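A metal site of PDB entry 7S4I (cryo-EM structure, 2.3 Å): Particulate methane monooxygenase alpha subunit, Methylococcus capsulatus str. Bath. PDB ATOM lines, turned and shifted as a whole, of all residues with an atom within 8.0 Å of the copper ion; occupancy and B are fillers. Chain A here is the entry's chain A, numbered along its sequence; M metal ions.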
ATOM      1  N   MET A  44      -1.884 -10.310 -23.600  1.00  0.00           N
ATOM      2  CA  MET A  44      -2.387 -11.667 -23.802  1.00  0.00           C
ATOM      3  C   MET A  44      -3.911 -11.692 -23.904  1.00  0.00           C
ATOM      4  O   MET A  44      -4.461 -12.386 -24.759  1.00  0.00           O
ATOM      5  CB  MET A  44      -1.924 -12.579 -22.666  1.00  0.00           C
ATOM      6  CG  MET A  44      -0.493 -13.036 -22.777  1.00  0.00           C
ATOM      7  SD  MET A  44       0.178 -13.581 -21.193  1.00  0.00           S
ATOM      8  CE  MET A  44       1.679 -14.376 -21.711  1.00  0.00           C
ATOM      9  N   ARG A  45      -4.604 -10.956 -23.048  1.00  0.00           N
ATOM     10  CA  ARG A  45      -6.056 -10.988 -23.029  1.00  0.00           C
ATOM     11  C   ARG A  45      -6.615  -9.600 -23.366  1.00  0.00           C
ATOM     12  O   ARG A  45      -7.141  -8.902 -22.510  1.00  0.00           O
ATOM     13  CB  ARG A  45      -6.544 -11.438 -21.651  1.00  0.00           C
ATOM     14  CG  ARG A  45      -5.580 -12.360 -20.920  1.00  0.00           C
ATOM     15  CD  ARG A  45      -5.666 -12.189 -19.402  1.00  0.00           C
ATOM     16  NE  ARG A  45      -7.023 -12.327 -18.903  1.00  0.00           N
ATOM     17  CZ  ARG A  45      -7.618 -13.491 -18.656  1.00  0.00           C
ATOM     18  NH1 ARG A  45      -6.999 -14.640 -18.867  1.00  0.00           N
ATOM     19  NH2 ARG A  45      -8.863 -13.499 -18.189  1.00  0.00           N
ATOM     20  N   THR A  46      -6.493  -9.213 -24.637  1.00  0.00           N
ATOM     21  CA  THR A  46      -7.381  -8.198 -25.190  1.00  0.00           C
ATOM     22  C   THR A  46      -7.964  -8.646 -26.518  1.00  0.00           C
ATOM     23  O   THR A  46      -9.181  -8.792 -26.676  1.00  0.00           O
ATOM     24  CB  THR A  46      -6.639  -6.868 -25.358  1.00  0.00           C
ATOM     25  OG1 THR A  46      -5.287  -7.113 -25.754  1.00  0.00           O
ATOM     26  CG2 THR A  46      -6.666  -6.082 -24.063  1.00  0.00           C
ATOM     27  N   ILE A  47      -7.080  -8.926 -27.478  1.00  0.00           N
ATOM     28  CA  ILE A  47      -7.426  -9.168 -28.871  1.00  0.00           C
ATOM     29  C   ILE A  47      -6.382 -10.103 -29.455  1.00  0.00           C
ATOM     30  O   ILE A  47      -5.182  -9.828 -29.353  1.00  0.00           O
ATOM     31  CB  ILE A  47      -7.513  -7.871 -29.690  1.00  0.00           C
ATOM     32  CG1 ILE A  47      -8.820  -7.133 -29.408  1.00  0.00           C
ATOM     33  CG2 ILE A  47      -7.372  -8.152 -31.170  1.00  0.00           C
ATOM     34  CD1 ILE A  47      -8.895  -5.772 -30.039  1.00  0.00           C
ATOM     35  N   HIS A  48      -6.816 -11.194 -30.059  1.00  0.00           N
ATOM     36  CA  HIS A  48      -5.919 -12.180 -30.647  1.00  0.00           C
ATOM     37  C   HIS A  48      -5.955 -12.048 -32.160  1.00  0.00           C
ATOM     38  O   HIS A  48      -6.998 -12.254 -32.782  1.00  0.00           O
ATOM     39  CB  HIS A  48      -6.296 -13.585 -30.204  1.00  0.00           C
ATOM     40  CG  HIS A  48      -6.362 -13.761 -28.717  1.00  0.00           C
ATOM     41  ND1 HIS A  48      -7.329 -14.510 -28.092  1.00  0.00           N
ATOM     42  CD2 HIS A  48      -5.578 -13.268 -27.733  1.00  0.00           C
ATOM     43  CE1 HIS A  48      -7.134 -14.476 -26.786  1.00  0.00           C
ATOM     44  NE2 HIS A  48      -6.076 -13.721 -26.547  1.00  0.00           N
ATOM     45  N   TRP A  49      -4.809 -11.704 -32.748  1.00  0.00           N
ATOM     46  CA  TRP A  49      -4.680 -11.560 -34.194  1.00  0.00           C
ATOM     47  C   TRP A  49      -4.164 -12.852 -34.788  1.00  0.00           C
ATOM     48  O   TRP A  49      -3.155 -13.399 -34.313  1.00  0.00           O
ATOM     49  CB  TRP A  49      -3.728 -10.415 -34.543  1.00  0.00           C
ATOM     50  CG  TRP A  49      -3.982  -9.133 -33.796  1.00  0.00           C
ATOM     51  CD1 TRP A  49      -3.597  -8.845 -32.520  1.00  0.00           C
ATOM     52  CD2 TRP A  49      -4.669  -7.976 -34.283  1.00  0.00           C
ATOM     53  NE1 TRP A  49      -4.003  -7.578 -32.185  1.00  0.00           N
ATOM     54  CE2 TRP A  49      -4.662  -7.021 -33.250  1.00  0.00           C
ATOM     55  CE3 TRP A  49      -5.287  -7.656 -35.492  1.00  0.00           C
ATOM     56  CZ2 TRP A  49      -5.253  -5.772 -33.389  1.00  0.00           C
ATOM     57  CZ3 TRP A  49      -5.868  -6.411 -35.631  1.00  0.00           C
ATOM     58  CH2 TRP A  49      -5.850  -5.479 -34.584  1.00  0.00           C
ATOM     59  N   TYR A  50      -4.842 -13.348 -35.821  1.00  0.00           N
ATOM     60  CA  TYR A  50      -4.401 -14.556 -36.501  1.00  0.00           C
ATOM     61  C   TYR A  50      -4.862 -14.503 -37.948  1.00  0.00           C
ATOM     62  O   TYR A  50      -5.645 -13.634 -38.337  1.00  0.00           O
ATOM     63  CB  TYR A  50      -4.891 -15.830 -35.796  1.00  0.00           C
ATOM     64  CG  TYR A  50      -6.392 -16.021 -35.824  1.00  0.00           C
ATOM     65  CD1 TYR A  50      -7.213 -15.342 -34.950  1.00  0.00           C
ATOM     66  CD2 TYR A  50      -6.975 -16.918 -36.721  1.00  0.00           C
ATOM     67  CE1 TYR A  50      -8.584 -15.528 -34.964  1.00  0.00           C
ATOM     68  CE2 TYR A  50      -8.337 -17.108 -36.736  1.00  0.00           C
ATOM     69  CZ  TYR A  50      -9.141 -16.411 -35.862  1.00  0.00           C
ATOM     70  OH  TYR A  50     -10.502 -16.601 -35.876  1.00  0.00           O
ATOM     71  N   PHE A  71      -9.140 -10.855 -36.183  1.00  0.00           N
ATOM     72  CA  PHE A  71      -8.902 -10.616 -34.777  1.00  0.00           C
ATOM     73  C   PHE A  71     -10.109 -11.063 -33.969  1.00  0.00           C
ATOM     74  O   PHE A  71     -11.255 -10.881 -34.399  1.00  0.00           O
ATOM     75  CB  PHE A  71      -8.567  -9.138 -34.483  1.00  0.00           C
ATOM     76  CG  PHE A  71      -9.682  -8.183 -34.803  1.00  0.00           C
ATOM     77  CD1 PHE A  71     -10.633  -7.850 -33.853  1.00  0.00           C
ATOM     78  CD2 PHE A  71      -9.757  -7.579 -36.055  1.00  0.00           C
ATOM     79  CE1 PHE A  71     -11.644  -6.962 -34.140  1.00  0.00           C
ATOM     80  CE2 PHE A  71     -10.772  -6.699 -36.347  1.00  0.00           C
ATOM     81  CZ  PHE A  71     -11.718  -6.383 -35.392  1.00  0.00           C
ATOM     82  N   HIS A  72      -9.843 -11.672 -32.819  1.00  0.00           N
ATOM     83  CA  HIS A  72     -10.884 -12.156 -31.921  1.00  0.00           C
ATOM     84  C   HIS A  72     -10.839 -11.350 -30.626  1.00  0.00           C
ATOM     85  O   HIS A  72      -9.780 -11.216 -30.012  1.00  0.00           O
ATOM     86  CB  HIS A  72     -10.703 -13.642 -31.627  1.00  0.00           C
ATOM     87  CG  HIS A  72     -11.633 -14.170 -30.585  1.00  0.00           C
ATOM     88  ND1 HIS A  72     -11.199 -14.641 -29.365  1.00  0.00           N
ATOM     89  CD2 HIS A  72     -12.981 -14.294 -30.578  1.00  0.00           C
ATOM     90  CE1 HIS A  72     -12.239 -15.042 -28.651  1.00  0.00           C
ATOM     91  NE2 HIS A  72     -13.332 -14.840 -29.364  1.00  0.00           N
ATOM     92  N   VAL A  73     -11.987 -10.813 -30.229  1.00  0.00           N
ATOM     93  CA  VAL A  73     -12.079 -10.061 -28.983  1.00  0.00           C
ATOM     94  C   VAL A  73     -12.244 -11.054 -27.838  1.00  0.00           C
ATOM     95  O   VAL A  73     -13.218 -11.808 -27.794  1.00  0.00           O
ATOM     96  CB  VAL A  73     -13.245  -9.065 -29.026  1.00  0.00           C
ATOM     97  CG1 VAL A  73     -13.196  -8.137 -27.831  1.00  0.00           C
ATOM     98  CG2 VAL A  73     -13.217  -8.271 -30.329  1.00  0.00           C
ATOM     99  N   PHE A  74     -11.291 -11.054 -26.914  1.00  0.00           N
ATOM    100  CA  PHE A  74     -11.265 -12.052 -25.850  1.00  0.00           C
ATOM    101  C   PHE A  74     -12.448 -11.858 -24.903  1.00  0.00           C
ATOM    102  O   PHE A  74     -12.810 -10.731 -24.556  1.00  0.00           O
ATOM    103  CB  PHE A  74      -9.946 -11.961 -25.087  1.00  0.00           C
ATOM    104  CG  PHE A  74      -9.812 -12.985 -24.004  1.00  0.00           C
ATOM    105  CD1 PHE A  74     -10.020 -14.324 -24.268  1.00  0.00           C
ATOM    106  CD2 PHE A  74      -9.491 -12.611 -22.711  1.00  0.00           C
ATOM    107  CE1 PHE A  74      -9.900 -15.272 -23.275  1.00  0.00           C
ATOM    108  CE2 PHE A  74      -9.358 -13.555 -21.714  1.00  0.00           C
ATOM    109  CZ  PHE A  74      -9.563 -14.885 -21.996  1.00  0.00           C
ATOM    110  N   GLU A  75     -13.040 -12.982 -24.482  1.00  0.00           N
ATOM    111  CA  GLU A  75     -14.188 -12.921 -23.578  1.00  0.00           C
ATOM    112  C   GLU A  75     -13.805 -12.354 -22.220  1.00  0.00           C
ATOM    113  O   GLU A  75     -14.555 -11.576 -21.633  1.00  0.00           O
ATOM    114  CB  GLU A  75     -14.804 -14.317 -23.417  1.00  0.00           C
ATOM    115  CG  GLU A  75     -15.605 -14.773 -24.620  1.00  0.00           C
ATOM    116  CD  GLU A  75     -14.737 -15.415 -25.692  1.00  0.00           C
ATOM    117  OE1 GLU A  75     -13.499 -15.440 -25.518  1.00  0.00           O
ATOM    118  OE2 GLU A  75     -15.298 -15.883 -26.702  1.00  0.00           O
ATOM    119  N   GLY A  76     -12.637 -12.730 -21.707  1.00  0.00           N
ATOM    120  CA  GLY A  76     -12.165 -12.212 -20.433  1.00  0.00           C
ATOM    121  C   GLY A  76     -11.521 -10.855 -20.562  1.00  0.00           C
ATOM    122  O   GLY A  76     -10.380 -10.649 -20.124  1.00  0.00           O
ATOM    123  N   GLY A 119     -16.035 -11.371 -27.503  1.00  0.00           N
ATOM    124  CA  GLY A 119     -16.227 -12.755 -27.874  1.00  0.00           C
ATOM    125  C   GLY A 119     -16.400 -12.991 -29.356  1.00  0.00           C
ATOM    126  O   GLY A 119     -16.414 -14.156 -29.774  1.00  0.00           O
ATOM    127  N   LYS A 120     -16.526 -11.942 -30.149  1.00  0.00           N
ATOM    128  CA  LYS A 120     -16.738 -12.082 -31.583  1.00  0.00           C
ATOM    129  C   LYS A 120     -15.403 -12.035 -32.328  1.00  0.00           C
ATOM    130  O   LYS A 120     -14.430 -11.418 -31.877  1.00  0.00           O
ATOM    131  CB  LYS A 120     -17.660 -10.986 -32.106  1.00  0.00           C
ATOM    132  CG  LYS A 120     -19.097 -11.109 -31.625  1.00  0.00           C
ATOM    133  CD  LYS A 120     -19.796 -12.284 -32.290  1.00  0.00           C
ATOM    134  CE  LYS A 120     -20.988 -12.746 -31.487  1.00  0.00           C
ATOM    135  NZ  LYS A 120     -21.882 -13.645 -32.273  1.00  0.00           N
ATOM    136  N   THR A 121     -15.373 -12.695 -33.477  1.00  0.00           N
ATOM    137  CA  THR A 121     -14.221 -12.687 -34.360  1.00  0.00           C
ATOM    138  C   THR A 121     -14.573 -11.879 -35.601  1.00  0.00           C
ATOM    139  O   THR A 121     -15.615 -12.110 -36.223  1.00  0.00           O
ATOM    140  CB  THR A 121     -13.809 -14.110 -34.764  1.00  0.00           C
ATOM    141  OG1 THR A 121     -13.514 -14.868 -33.577  1.00  0.00           O
ATOM    142  CG2 THR A 121     -12.584 -14.076 -35.656  1.00  0.00           C
ATOM    143  N   TYR A 318      -0.732 -19.557 -29.903  1.00  0.00           N
ATOM    144  CA  TYR A 318      -0.559 -18.119 -30.034  1.00  0.00           C
ATOM    145  C   TYR A 318      -1.014 -17.480 -28.724  1.00  0.00           C
ATOM    146  O   TYR A 318      -2.145 -17.702 -28.290  1.00  0.00           O
ATOM    147  CB  TYR A 318      -1.365 -17.586 -31.224  1.00  0.00           C
ATOM    148  CG  TYR A 318      -1.576 -16.091 -31.285  1.00  0.00           C
ATOM    149  CD1 TYR A 318      -2.589 -15.471 -30.549  1.00  0.00           C
ATOM    150  CD2 TYR A 318      -0.772 -15.294 -32.094  1.00  0.00           C
ATOM    151  CE1 TYR A 318      -2.776 -14.113 -30.613  1.00  0.00           C
ATOM    152  CE2 TYR A 318      -0.969 -13.932 -32.158  1.00  0.00           C
ATOM    153  CZ  TYR A 318      -1.972 -13.344 -31.413  1.00  0.00           C
ATOM    154  OH  TYR A 318      -2.160 -11.987 -31.476  1.00  0.00           O
ATOM    155  N   THR A 319      -0.138 -16.691 -28.102  1.00  0.00           N
ATOM    156  CA  THR A 319      -0.446 -16.088 -26.805  1.00  0.00           C
ATOM    157  C   THR A 319      -0.565 -14.575 -26.898  1.00  0.00           C
ATOM    158  O   THR A 319      -1.622 -14.024 -26.568  1.00  0.00           O
ATOM    159  CB  THR A 319       0.593 -16.514 -25.759  1.00  0.00           C
ATOM    160  OG1 THR A 319       0.439 -15.702 -24.585  1.00  0.00           O
ATOM    161  CG2 THR A 319       2.010 -16.389 -26.298  1.00  0.00           C
ATOM    162  N   ALA A 388      -4.051 -15.721 -21.694  1.00  0.00           N
ATOM    163  CA  ALA A 388      -5.018 -16.218 -22.655  1.00  0.00           C
ATOM    164  C   ALA A 388      -4.296 -16.427 -23.979  1.00  0.00           C
ATOM    165  O   ALA A 388      -3.271 -15.800 -24.249  1.00  0.00           O
ATOM    166  CB  ALA A 388      -6.199 -15.265 -22.832  1.00  0.00           C
ATOM    167  N   GLY A 389      -4.853 -17.309 -24.809  1.00  0.00           N
ATOM    168  CA  GLY A 389      -4.233 -17.589 -26.083  1.00  0.00           C
ATOM    169  C   GLY A 389      -5.152 -18.385 -26.983  1.00  0.00           C
ATOM    170  O   GLY A 389      -6.306 -18.643 -26.647  1.00  0.00           O
ATOM    171  N   LEU A 390      -4.613 -18.767 -28.139  1.00  0.00           N
ATOM    172  CA  LEU A 390      -5.321 -19.571 -29.105  1.00  0.00           C
ATOM    173  C   LEU A 390      -4.515 -20.824 -29.408  1.00  0.00           C
ATOM    174  O   LEU A 390      -3.309 -20.742 -29.647  1.00  0.00           O
ATOM    175  CB  LEU A 390      -5.575 -18.791 -30.409  1.00  0.00           C
ATOM    176  CG  LEU A 390      -6.402 -17.513 -30.321  1.00  0.00           C
ATOM    177  CD1 LEU A 390      -6.508 -16.880 -31.698  1.00  0.00           C
ATOM    178  CD2 LEU A 390      -7.786 -17.807 -29.752  1.00  0.00           C
ATOM    179  N   VAL A 402      -9.673 -23.771 -34.260  1.00  0.00           N
ATOM    180  CA  VAL A 402      -9.179 -22.741 -33.352  1.00  0.00           C
ATOM    181  C   VAL A 402      -9.939 -22.866 -32.041  1.00  0.00           C
ATOM    182  O   VAL A 402     -11.169 -22.756 -32.019  1.00  0.00           O
ATOM    183  CB  VAL A 402      -9.332 -21.331 -33.930  1.00  0.00           C
ATOM    184  CG1 VAL A 402      -8.651 -20.313 -33.039  1.00  0.00           C
ATOM    185  CG2 VAL A 402      -8.767 -21.273 -35.339  1.00  0.00           C
ATOM    186  N   VAL A 403      -9.211 -23.094 -30.950  1.00  0.00           N
ATOM    187  CA  VAL A 403      -9.799 -23.126 -29.622  1.00  0.00           C
ATOM    188  C   VAL A 403      -9.058 -22.121 -28.749  1.00  0.00           C
ATOM    189  O   VAL A 403      -7.850 -21.891 -28.910  1.00  0.00           O
ATOM    190  CB  VAL A 403      -9.775 -24.540 -28.990  1.00  0.00           C
ATOM    191  CG1 VAL A 403     -10.200 -25.587 -30.006  1.00  0.00           C
ATOM    192  CG2 VAL A 403      -8.405 -24.861 -28.428  1.00  0.00           C
ATOM    193  N   GLN A 404      -9.790 -21.489 -27.847  1.00  0.00           N
ATOM    194  CA  GLN A 404      -9.260 -20.449 -26.983  1.00  0.00           C
ATOM    195  C   GLN A 404      -9.091 -21.000 -25.579  1.00  0.00           C
ATOM    196  O   GLN A 404      -9.968 -21.683 -25.054  1.00  0.00           O
ATOM    197  CB  GLN A 404     -10.171 -19.227 -26.979  1.00  0.00           C
ATOM    198  CG  GLN A 404      -9.728 -18.134 -26.040  1.00  0.00           C
ATOM    199  CD  GLN A 404     -10.423 -16.825 -26.337  1.00  0.00           C
ATOM    200  OE1 GLN A 404      -9.850 -15.929 -26.965  1.00  0.00           O
ATOM    201  NE2 GLN A 404     -11.669 -16.694 -25.886  1.00  0.00           N
ATOM    202  N   ILE A 405      -7.948 -20.697 -24.963  1.00  0.00           N
ATOM    203  CA  ILE A 405      -7.633 -21.141 -23.619  1.00  0.00           C
ATOM    204  C   ILE A 405      -7.253 -19.931 -22.772  1.00  0.00           C
ATOM    205  O   ILE A 405      -6.632 -18.990 -23.270  1.00  0.00           O
ATOM    206  CB  ILE A 405      -6.508 -22.190 -23.607  1.00  0.00           C
ATOM    207  CG1 ILE A 405      -5.271 -21.662 -24.340  1.00  0.00           C
ATOM    208  CG2 ILE A 405      -6.988 -23.493 -24.225  1.00  0.00           C
ATOM    209  CD1 ILE A 405      -4.025 -22.466 -24.084  1.00  0.00           C
HETATM  210 CU    CU M   1      -9.325 -14.236 -28.575  1.00  0.00          CU
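NE2 of His 48 is in hydrogen-bond range of O of Met 44 (2.8 Å).
NE2 of His 72 is in hydrogen-bond range of OE2 of Glu 75 (3.5 Å).
O of Gly 119 sits at hydrogen-bond distance from NE2 of His 72, at 3.2 Å.
N of Phe 74 sits at hydrogen-bond distance from O of Thr 46.
Phe 74 touches the copper ion (CA to CU, 3.99 Å).
Of the 25 residues printed, 4 come within 4 Å of the copper ion.
The copper ion is bound by a ring nitrogen (ND1) of His 48 (2.1 Å), a ring nitrogen (ND1) of His 72 (2.1 Å) and the side-chain amide oxygen (OE1) of Gln 404 (2.4 Å).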
